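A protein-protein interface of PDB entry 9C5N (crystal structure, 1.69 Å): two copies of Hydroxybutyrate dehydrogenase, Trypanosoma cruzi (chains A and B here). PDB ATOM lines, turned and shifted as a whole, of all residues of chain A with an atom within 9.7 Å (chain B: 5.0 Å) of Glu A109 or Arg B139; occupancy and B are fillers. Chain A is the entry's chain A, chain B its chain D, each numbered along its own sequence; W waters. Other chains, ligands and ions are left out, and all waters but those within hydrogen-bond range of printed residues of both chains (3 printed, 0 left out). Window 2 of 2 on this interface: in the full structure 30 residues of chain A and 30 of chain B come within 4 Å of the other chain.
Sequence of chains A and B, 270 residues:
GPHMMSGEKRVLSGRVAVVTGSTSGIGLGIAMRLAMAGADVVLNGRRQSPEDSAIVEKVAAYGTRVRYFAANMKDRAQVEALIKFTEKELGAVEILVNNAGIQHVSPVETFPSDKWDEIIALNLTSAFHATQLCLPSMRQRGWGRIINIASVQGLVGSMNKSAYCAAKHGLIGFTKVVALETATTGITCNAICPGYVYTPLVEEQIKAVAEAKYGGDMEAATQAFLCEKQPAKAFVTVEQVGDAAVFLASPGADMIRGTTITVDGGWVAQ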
ATOM      1  N   VAL A 105     -25.287  10.427  -4.045  1.00  0.00           N
ATOM      2  CA  VAL A 105     -23.951  11.015  -4.088  1.00  0.00           C
ATOM      3  C   VAL A 105     -24.061  12.482  -3.697  1.00  0.00           C
ATOM      4  O   VAL A 105     -24.781  13.257  -4.339  1.00  0.00           O
ATOM      5  CB  VAL A 105     -23.323  10.861  -5.484  1.00  0.00           C
ATOM      6  CG1 VAL A 105     -21.926  11.468  -5.533  1.00  0.00           C
ATOM      7  CG2 VAL A 105     -23.298   9.365  -5.898  1.00  0.00           C
ATOM      8  N   SER A 106     -23.335  12.865  -2.638  1.00  0.00           N
ATOM      9  CA  SER A 106     -23.322  14.237  -2.152  1.00  0.00           C
ATOM     10  C   SER A 106     -22.144  14.396  -1.214  1.00  0.00           C
ATOM     11  O   SER A 106     -21.863  13.458  -0.449  1.00  0.00           O
ATOM     12  CB  SER A 106     -24.612  14.566  -1.393  1.00  0.00           C
ATOM     13  OG  SER A 106     -24.498  15.829  -0.755  1.00  0.00           O
ATOM     14  N   PRO A 107     -21.477  15.549  -1.190  1.00  0.00           N
ATOM     15  CA  PRO A 107     -20.545  15.836  -0.091  1.00  0.00           C
ATOM     16  C   PRO A 107     -21.270  15.766   1.251  1.00  0.00           C
ATOM     17  O   PRO A 107     -22.482  15.972   1.333  1.00  0.00           O
ATOM     18  CB  PRO A 107     -20.050  17.256  -0.394  1.00  0.00           C
ATOM     19  CG  PRO A 107     -20.324  17.462  -1.830  1.00  0.00           C
ATOM     20  CD  PRO A 107     -21.534  16.638  -2.174  1.00  0.00           C
ATOM     21  N   VAL A 108     -20.504  15.483   2.312  1.00  0.00           N
ATOM     22  CA  VAL A 108     -21.084  15.310   3.642  1.00  0.00           C
ATOM     23  C   VAL A 108     -21.815  16.570   4.087  1.00  0.00           C
ATOM     24  O   VAL A 108     -22.875  16.494   4.714  1.00  0.00           O
ATOM     25  CB  VAL A 108     -19.994  14.924   4.656  1.00  0.00           C
ATOM     26  CG1 VAL A 108     -20.559  14.897   6.083  1.00  0.00           C
ATOM     27  CG2 VAL A 108     -19.454  13.576   4.341  1.00  0.00           C
ATOM     28  N   GLU A 109     -21.264  17.749   3.769  1.00  0.00           N
ATOM     29  CA  GLU A 109     -21.802  18.989   4.316  1.00  0.00           C
ATOM     30  C   GLU A 109     -23.232  19.239   3.878  1.00  0.00           C
ATOM     31  O   GLU A 109     -23.993  19.905   4.589  1.00  0.00           O
ATOM     32  CB  GLU A 109     -20.958  20.194   3.895  1.00  0.00           C
ATOM     33  CG  GLU A 109     -19.569  20.245   4.512  1.00  0.00           C
ATOM     34  CD  GLU A 109     -18.527  19.475   3.716  1.00  0.00           C
ATOM     35  OE1 GLU A 109     -18.892  18.821   2.710  1.00  0.00           O
ATOM     36  OE2 GLU A 109     -17.335  19.519   4.109  1.00  0.00           O
ATOM     37  N   THR A 110     -23.584  18.815   2.667  1.00  0.00           N
ATOM     38  CA  THR A 110     -24.893  19.092   2.095  1.00  0.00           C
ATOM     39  C   THR A 110     -25.725  17.825   1.942  1.00  0.00           C
ATOM     40  O   THR A 110     -26.788  17.870   1.309  1.00  0.00           O
ATOM     41  CB  THR A 110     -24.741  19.775   0.736  1.00  0.00           C
ATOM     42  OG1 THR A 110     -23.868  18.984  -0.079  1.00  0.00           O
ATOM     43  CG2 THR A 110     -24.150  21.177   0.895  1.00  0.00           C
ATOM     44  N   PHE A 111     -25.269  16.708   2.505  1.00  0.00           N
ATOM     45  CA  PHE A 111     -25.979  15.439   2.387  1.00  0.00           C
ATOM     46  C   PHE A 111     -27.362  15.566   3.023  1.00  0.00           C
ATOM     47  O   PHE A 111     -27.456  15.885   4.220  1.00  0.00           O
ATOM     48  CB  PHE A 111     -25.199  14.314   3.057  1.00  0.00           C
ATOM     49  CG  PHE A 111     -25.458  12.984   2.434  1.00  0.00           C
ATOM     50  CD1 PHE A 111     -26.680  12.355   2.606  1.00  0.00           C
ATOM     51  CD2 PHE A 111     -24.500  12.386   1.633  1.00  0.00           C
ATOM     52  CE1 PHE A 111     -26.925  11.138   2.008  1.00  0.00           C
ATOM     53  CE2 PHE A 111     -24.736  11.188   1.026  1.00  0.00           C
ATOM     54  CZ  PHE A 111     -25.949  10.550   1.202  1.00  0.00           C
ATOM     55  N   PRO A 112     -28.448  15.363   2.274  1.00  0.00           N
ATOM     56  CA  PRO A 112     -29.778  15.573   2.855  1.00  0.00           C
ATOM     57  C   PRO A 112     -30.071  14.557   3.945  1.00  0.00           C
ATOM     58  O   PRO A 112     -29.790  13.365   3.810  1.00  0.00           O
ATOM     59  CB  PRO A 112     -30.727  15.408   1.655  1.00  0.00           C
ATOM     60  CG  PRO A 112     -29.871  15.660   0.455  1.00  0.00           C
ATOM     61  CD  PRO A 112     -28.528  15.092   0.826  1.00  0.00           C
ATOM     62  N   SER A 113     -30.672  15.051   5.029  1.00  0.00           N
ATOM     63  CA  SER A 113     -30.946  14.187   6.171  1.00  0.00           C
ATOM     64  C   SER A 113     -31.890  13.047   5.797  1.00  0.00           C
ATOM     65  O   SER A 113     -31.680  11.904   6.217  1.00  0.00           O
ATOM     66  CB  SER A 113     -31.521  15.014   7.321  1.00  0.00           C
ATOM     67  OG  SER A 113     -30.512  15.816   7.919  1.00  0.00           O
ATOM     68  N   TRP A 116     -29.936  10.386   3.923  1.00  0.00           N
ATOM     69  CA  TRP A 116     -29.096   9.634   4.849  1.00  0.00           C
ATOM     70  C   TRP A 116     -29.930   8.554   5.530  1.00  0.00           C
ATOM     71  O   TRP A 116     -29.591   7.365   5.495  1.00  0.00           O
ATOM     72  CB  TRP A 116     -28.459  10.583   5.897  1.00  0.00           C
ATOM     73  CG  TRP A 116     -27.702   9.814   6.967  1.00  0.00           C
ATOM     74  CD1 TRP A 116     -28.245   9.231   8.089  1.00  0.00           C
ATOM     75  CD2 TRP A 116     -26.295   9.532   7.018  1.00  0.00           C
ATOM     76  NE1 TRP A 116     -27.267   8.599   8.812  1.00  0.00           N
ATOM     77  CE2 TRP A 116     -26.063   8.767   8.179  1.00  0.00           C
ATOM     78  CE3 TRP A 116     -25.207   9.859   6.205  1.00  0.00           C
ATOM     79  CZ2 TRP A 116     -24.794   8.317   8.535  1.00  0.00           C
ATOM     80  CZ3 TRP A 116     -23.952   9.410   6.560  1.00  0.00           C
ATOM     81  CH2 TRP A 116     -23.754   8.631   7.708  1.00  0.00           C
ATOM     82  N   MET A 159     -15.240   9.219  -1.800  1.00  0.00           N
ATOM     83  CA  MET A 159     -15.743  10.581  -1.648  1.00  0.00           C
ATOM     84  C   MET A 159     -17.210  10.666  -2.051  1.00  0.00           C
ATOM     85  O   MET A 159     -17.645  10.041  -3.026  1.00  0.00           O
ATOM     86  CB  MET A 159     -14.933  11.556  -2.499  1.00  0.00           C
ATOM     87  CG  MET A 159     -13.587  11.862  -1.898  1.00  0.00           C
ATOM     88  SD  MET A 159     -12.709  13.169  -2.744  1.00  0.00           S
ATOM     89  CE  MET A 159     -12.159  12.316  -4.184  1.00  0.00           C
ATOM     90  N   ASN A 160     -17.974  11.429  -1.267  1.00  0.00           N
ATOM     91  CA  ASN A 160     -19.347  11.799  -1.600  1.00  0.00           C
ATOM     92  C   ASN A 160     -20.323  10.641  -1.473  1.00  0.00           C
ATOM     93  O   ASN A 160     -21.450  10.733  -1.942  1.00  0.00           O
ATOM     94  CB  ASN A 160     -19.407  12.404  -3.002  1.00  0.00           C
ATOM     95  CG  ASN A 160     -18.520  13.629  -3.132  1.00  0.00           C
ATOM     96  OD1 ASN A 160     -18.382  14.418  -2.189  1.00  0.00           O
ATOM     97  ND2 ASN A 160     -17.868  13.761  -4.273  1.00  0.00           N
ATOM     98  N   LYS A 161     -19.930   9.564  -0.799  1.00  0.00           N
ATOM     99  CA  LYS A 161     -20.795   8.412  -0.552  1.00  0.00           C
ATOM    100  C   LYS A 161     -20.829   8.066   0.930  1.00  0.00           C
ATOM    101  O   LYS A 161     -20.791   6.893   1.320  1.00  0.00           O
ATOM    102  CB  LYS A 161     -20.340   7.218  -1.389  1.00  0.00           C
ATOM    103  CG  LYS A 161     -20.604   7.462  -2.877  1.00  0.00           C
ATOM    104  CD  LYS A 161     -19.949   6.388  -3.772  1.00  0.00           C
ATOM    105  CE  LYS A 161     -20.292   6.619  -5.241  1.00  0.00           C
ATOM    106  NZ  LYS A 161     -19.655   5.615  -6.153  1.00  0.00           N
ATOM    107  N   SER A 162     -20.928   9.083   1.793  1.00  0.00           N
ATOM    108  CA  SER A 162     -20.817   8.820   3.226  1.00  0.00           C
ATOM    109  C   SER A 162     -21.914   7.882   3.725  1.00  0.00           C
ATOM    110  O   SER A 162     -21.640   6.936   4.476  1.00  0.00           O
ATOM    111  CB  SER A 162     -20.840  10.141   4.002  1.00  0.00           C
ATOM    112  OG  SER A 162     -21.973  10.934   3.698  1.00  0.00           O
ATOM    113  N   GLN B 132     -21.482  17.112  10.023  1.00  0.00           N
ATOM    114  CA  GLN B 132     -22.062  18.017   9.045  1.00  0.00           C
ATOM    115  C   GLN B 132     -22.100  19.441   9.572  1.00  0.00           C
ATOM    116  O   GLN B 132     -21.800  20.389   8.839  1.00  0.00           O
ATOM    117  CB  GLN B 132     -23.466  17.524   8.698  1.00  0.00           C
ATOM    118  CG  GLN B 132     -24.157  18.248   7.608  1.00  0.00           C
ATOM    119  CD  GLN B 132     -25.400  17.503   7.157  1.00  0.00           C
ATOM    120  OE1 GLN B 132     -26.386  17.416   7.884  1.00  0.00           O
ATOM    121  NE2 GLN B 132     -25.348  16.951   5.964  1.00  0.00           N
ATOM    122  N   LEU B 135     -18.118  20.862   9.977  1.00  0.00           N
ATOM    123  CA  LEU B 135     -17.171  20.932   8.870  1.00  0.00           C
ATOM    124  C   LEU B 135     -17.070  22.298   8.204  1.00  0.00           C
ATOM    125  O   LEU B 135     -15.947  22.684   7.836  1.00  0.00           O
ATOM    126  CB  LEU B 135     -17.510  19.863   7.821  1.00  0.00           C
ATOM    127  CG  LEU B 135     -16.954  18.464   8.081  1.00  0.00           C
ATOM    128  CD1 LEU B 135     -17.577  17.437   7.099  1.00  0.00           C
ATOM    129  CD2 LEU B 135     -15.429  18.432   7.959  1.00  0.00           C
ATOM    130  N   PRO B 136     -18.154  23.051   7.972  1.00  0.00           N
ATOM    131  CA  PRO B 136     -17.993  24.331   7.253  1.00  0.00           C
ATOM    132  C   PRO B 136     -17.058  25.304   7.948  1.00  0.00           C
ATOM    133  O   PRO B 136     -16.219  25.931   7.286  1.00  0.00           O
ATOM    134  CB  PRO B 136     -19.432  24.863   7.167  1.00  0.00           C
ATOM    135  CG  PRO B 136     -20.271  23.605   7.191  1.00  0.00           C
ATOM    136  CD  PRO B 136     -19.575  22.698   8.147  1.00  0.00           C
ATOM    137  N   SER B 137     -17.171  25.438   9.271  1.00  0.00           N
ATOM    138  CA  SER B 137     -16.257  26.283  10.020  1.00  0.00           C
ATOM    139  C   SER B 137     -14.834  25.757   9.944  1.00  0.00           C
ATOM    140  O   SER B 137     -13.892  26.534   9.777  1.00  0.00           O
ATOM    141  CB  SER B 137     -16.707  26.353  11.475  1.00  0.00           C
ATOM    142  OG  SER B 137     -15.786  27.089  12.247  1.00  0.00           O
ATOM    143  N   MET B 138     -14.648  24.443  10.105  1.00  0.00           N
ATOM    144  CA  MET B 138     -13.298  23.887  10.042  1.00  0.00           C
ATOM    145  C   MET B 138     -12.650  24.191   8.693  1.00  0.00           C
ATOM    146  O   MET B 138     -11.465  24.545   8.628  1.00  0.00           O
ATOM    147  CB  MET B 138     -13.325  22.387  10.295  1.00  0.00           C
ATOM    148  CG  MET B 138     -13.622  22.013  11.726  1.00  0.00           C
ATOM    149  SD  MET B 138     -13.896  20.243  11.860  1.00  0.00           S
ATOM    150  CE  MET B 138     -14.159  20.093  13.641  1.00  0.00           C
ATOM    151  N   ARG B 139     -13.410  24.061   7.600  1.00  0.00           N
ATOM    152  CA  ARG B 139     -12.858  24.375   6.282  1.00  0.00           C
ATOM    153  C   ARG B 139     -12.470  25.844   6.176  1.00  0.00           C
ATOM    154  O   ARG B 139     -11.394  26.175   5.662  1.00  0.00           O
ATOM    155  CB  ARG B 139     -13.856  24.015   5.181  1.00  0.00           C
ATOM    156  CG  ARG B 139     -14.048  22.522   4.970  1.00  0.00           C
ATOM    157  CD  ARG B 139     -14.994  22.271   3.781  1.00  0.00           C
ATOM    158  NE  ARG B 139     -15.133  20.853   3.445  1.00  0.00           N
ATOM    159  CZ  ARG B 139     -14.249  20.167   2.731  1.00  0.00           C
ATOM    160  NH1 ARG B 139     -13.106  20.709   2.347  1.00  0.00           N
ATOM    161  NH2 ARG B 139     -14.541  18.919   2.362  1.00  0.00           N
ATOM    162  N   GLN B 140     -13.337  26.737   6.650  1.00  0.00           N
ATOM    163  CA  GLN B 140     -13.036  28.160   6.617  1.00  0.00           C
ATOM    164  C   GLN B 140     -11.769  28.474   7.396  1.00  0.00           C
ATOM    165  O   GLN B 140     -10.982  29.333   6.986  1.00  0.00           O
ATOM    166  CB  GLN B 140     -14.197  28.961   7.206  1.00  0.00           C
ATOM    167  CG  GLN B 140     -15.294  29.316   6.275  1.00  0.00           C
ATOM    168  CD  GLN B 140     -16.057  30.525   6.801  1.00  0.00           C
ATOM    169  OE1 GLN B 140     -16.382  30.584   7.987  1.00  0.00           O
ATOM    170  NE2 GLN B 140     -16.304  31.510   5.934  1.00  0.00           N
ATOM    171  N   ARG B 141     -11.585  27.828   8.553  1.00  0.00           N
ATOM    172  CA  ARG B 141     -10.454  28.106   9.433  1.00  0.00           C
ATOM    173  C   ARG B 141      -9.195  27.332   9.071  1.00  0.00           C
ATOM    174  O   ARG B 141      -8.134  27.612   9.649  1.00  0.00           O
ATOM    175  CB  ARG B 141     -10.824  27.808  10.889  1.00  0.00           C
ATOM    176  CG  ARG B 141     -11.922  28.704  11.417  1.00  0.00           C
ATOM    177  CD  ARG B 141     -12.282  28.335  12.847  1.00  0.00           C
ATOM    178  NE  ARG B 141     -11.450  28.983  13.857  1.00  0.00           N
ATOM    179  CZ  ARG B 141     -11.720  30.150  14.436  1.00  0.00           C
ATOM    180  NH1 ARG B 141     -12.741  30.901  14.052  1.00  0.00           N
ATOM    181  NH2 ARG B 141     -10.965  30.563  15.446  1.00  0.00           N
ATOM    182  N   GLY B 142      -9.275  26.408   8.117  1.00  0.00           N
ATOM    183  CA  GLY B 142      -8.104  25.683   7.668  1.00  0.00           C
ATOM    184  C   GLY B 142      -7.592  24.606   8.596  1.00  0.00           C
ATOM    185  O   GLY B 142      -6.446  24.182   8.448  1.00  0.00           O
ATOM    186  N   GLU B 181     -12.917  13.249   1.799  1.00  0.00           N
ATOM    187  CA  GLU B 181     -13.462  14.519   1.342  1.00  0.00           C
ATOM    188  C   GLU B 181     -12.681  15.713   1.867  1.00  0.00           C
ATOM    189  O   GLU B 181     -12.830  16.811   1.318  1.00  0.00           O
ATOM    190  CB  GLU B 181     -14.926  14.650   1.760  1.00  0.00           C
ATOM    191  CG  GLU B 181     -15.822  13.651   1.066  1.00  0.00           C
ATOM    192  CD  GLU B 181     -17.288  13.830   1.383  1.00  0.00           C
ATOM    193  OE1 GLU B 181     -17.690  14.873   1.971  1.00  0.00           O
ATOM    194  OE2 GLU B 181     -18.054  12.910   1.013  1.00  0.00           O
ATOM    195  N   THR B 182     -11.866  15.534   2.914  1.00  0.00           N
ATOM    196  CA  THR B 182     -11.055  16.606   3.485  1.00  0.00           C
ATOM    197  C   THR B 182      -9.560  16.362   3.316  1.00  0.00           C
ATOM    198  O   THR B 182      -8.758  17.062   3.933  1.00  0.00           O
ATOM    199  CB  THR B 182     -11.360  16.792   4.983  1.00  0.00           C
ATOM    200  OG1 THR B 182     -11.137  15.555   5.674  1.00  0.00           O
ATOM    201  CG2 THR B 182     -12.784  17.240   5.203  1.00  0.00           C
ATOM    202  N   THR B 185      -6.890  19.211   2.910  1.00  0.00           N
ATOM    203  CA  THR B 185      -7.103  20.327   3.822  1.00  0.00           C
ATOM    204  C   THR B 185      -6.399  20.050   5.153  1.00  0.00           C
ATOM    205  O   THR B 185      -5.877  18.954   5.402  1.00  0.00           O
ATOM    206  CB  THR B 185      -8.593  20.557   4.116  1.00  0.00           C
ATOM    207  OG1 THR B 185      -9.052  19.559   5.028  1.00  0.00           O
ATOM    208  CG2 THR B 185      -9.451  20.471   2.883  1.00  0.00           C
ATOM    209  N   ILE B 187      -7.952  19.509   7.809  1.00  0.00           N
ATOM    210  CA  ILE B 187      -8.919  18.765   8.611  1.00  0.00           C
ATOM    211  C   ILE B 187      -8.620  17.282   8.458  1.00  0.00           C
ATOM    212  O   ILE B 187      -8.525  16.784   7.331  1.00  0.00           O
ATOM    213  CB  ILE B 187     -10.364  19.025   8.160  1.00  0.00           C
ATOM    214  CG1 ILE B 187     -10.760  20.490   8.244  1.00  0.00           C
ATOM    215  CG2 ILE B 187     -11.336  18.153   8.974  1.00  0.00           C
ATOM    216  CD1 ILE B 187     -11.962  20.799   7.350  1.00  0.00           C
HETATM  217  O   HOH W   1     -20.628  12.042   1.492  1.00  0.00           O
HETATM  218  O   HOH W   2     -23.211  21.798   7.007  1.00  0.00           O
HETATM  219  O   HOH W   3     -16.972  17.355   1.715  1.00  0.00           O
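N of Phe A111 lies within hydrogen-bond range of OG of Ser A106 (3.5 Å).
The backbone NH of Ser A106 sits at hydrogen-bond distance from the backbone carbonyl oxygen of Asn A160.
The backbone carbonyl oxygen (O) of Glu B181 is in hydrogen-bond range of the guanidinium group (NH2) of Arg B139.
The side-chain amide nitrogen (NE2) of Gln B132 is in hydrogen-bond range of the backbone carbonyl oxygen (O) of Val A108.
NE2 of Gln B132 is in hydrogen-bond range of O of Phe A111, at 2.9 Å.
The side-chain carboxylate (OE2) of Glu A109 lies within salt-bridge range of the guanidinium group (NE) of Arg B139 (2.7 Å).
The backbone NH of Asn A160 lies within hydrogen-bond range of the side-chain carboxylate of Glu B181, 2.7 Å away.
The side-chain carboxylate (OE1) of Glu B181 is in hydrogen-bond range of the backbone NH (N) of Val A108, at 2.9 Å.
CA of Pro A107 touches OE1 of Glu B181, at 3.7 Å.
Gln B132 touches Glu A109 (CG to O, 3.4 Å).
Leu B135 touches Glu A109.
OE2 of Glu B181 touches C of Met A159, 3.9 Å away.
Water W3 lies within hydrogen-bond range of the side-chain carboxylate (OE1) of Glu B181, the side-chain carboxylate (OE1) of Glu A109 and the guanidinium group (NH2) of Arg B139.
Water W1 lies within hydrogen-bond range of O of Ser A106 (2.7 Å), OE2 of Glu B181 (2.8 Å), OG of Ser A162 (2.8 Å) and N of Lys A161 (3.4 Å).
Water W2 lies within hydrogen-bond range of the backbone carbonyl oxygen (O) of Gln B132 (2.7 Å) and the backbone carbonyl oxygen (O) of Glu A109 (3.2 Å).
No position is printed for both chains.
Of the 9 pairs that touch across the chains among the printed residues, none has its exchanged pair printed and touching as well.
Of the 14 printed residues of chain A, 6 touch a printed residue of chain B.
Of the 13 printed residues of chain B, 4 touch a printed residue of chain A.
Hydrophobic or aromatic side chains of chain B that line the printed part of chain A: Leu B135.
Among the printed residues, 9 pairs touch across the chains.
Of chain A, only Glu A109 (2.7 Å) comes within 4 Å of Arg B139.
Printed residues of chain B within 4 Å of Pro A107: Glu B181.
Printed residues of chain B within 4 Å of Val A108: Gln B132 (2.8 Å) and Glu B181 (2.9 Å).
Printed residues of chain B within 4 Å of Phe A111: Gln B132.
Printed residues of chain A within 4 Å of Gln B132: Val A108, Glu A109 and Phe A111.
Pro A112 touches none of the printed residues of chain B.
The nearest printed residue of chain B that does not touch Val A108 is Leu B135 (4.05 Å).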
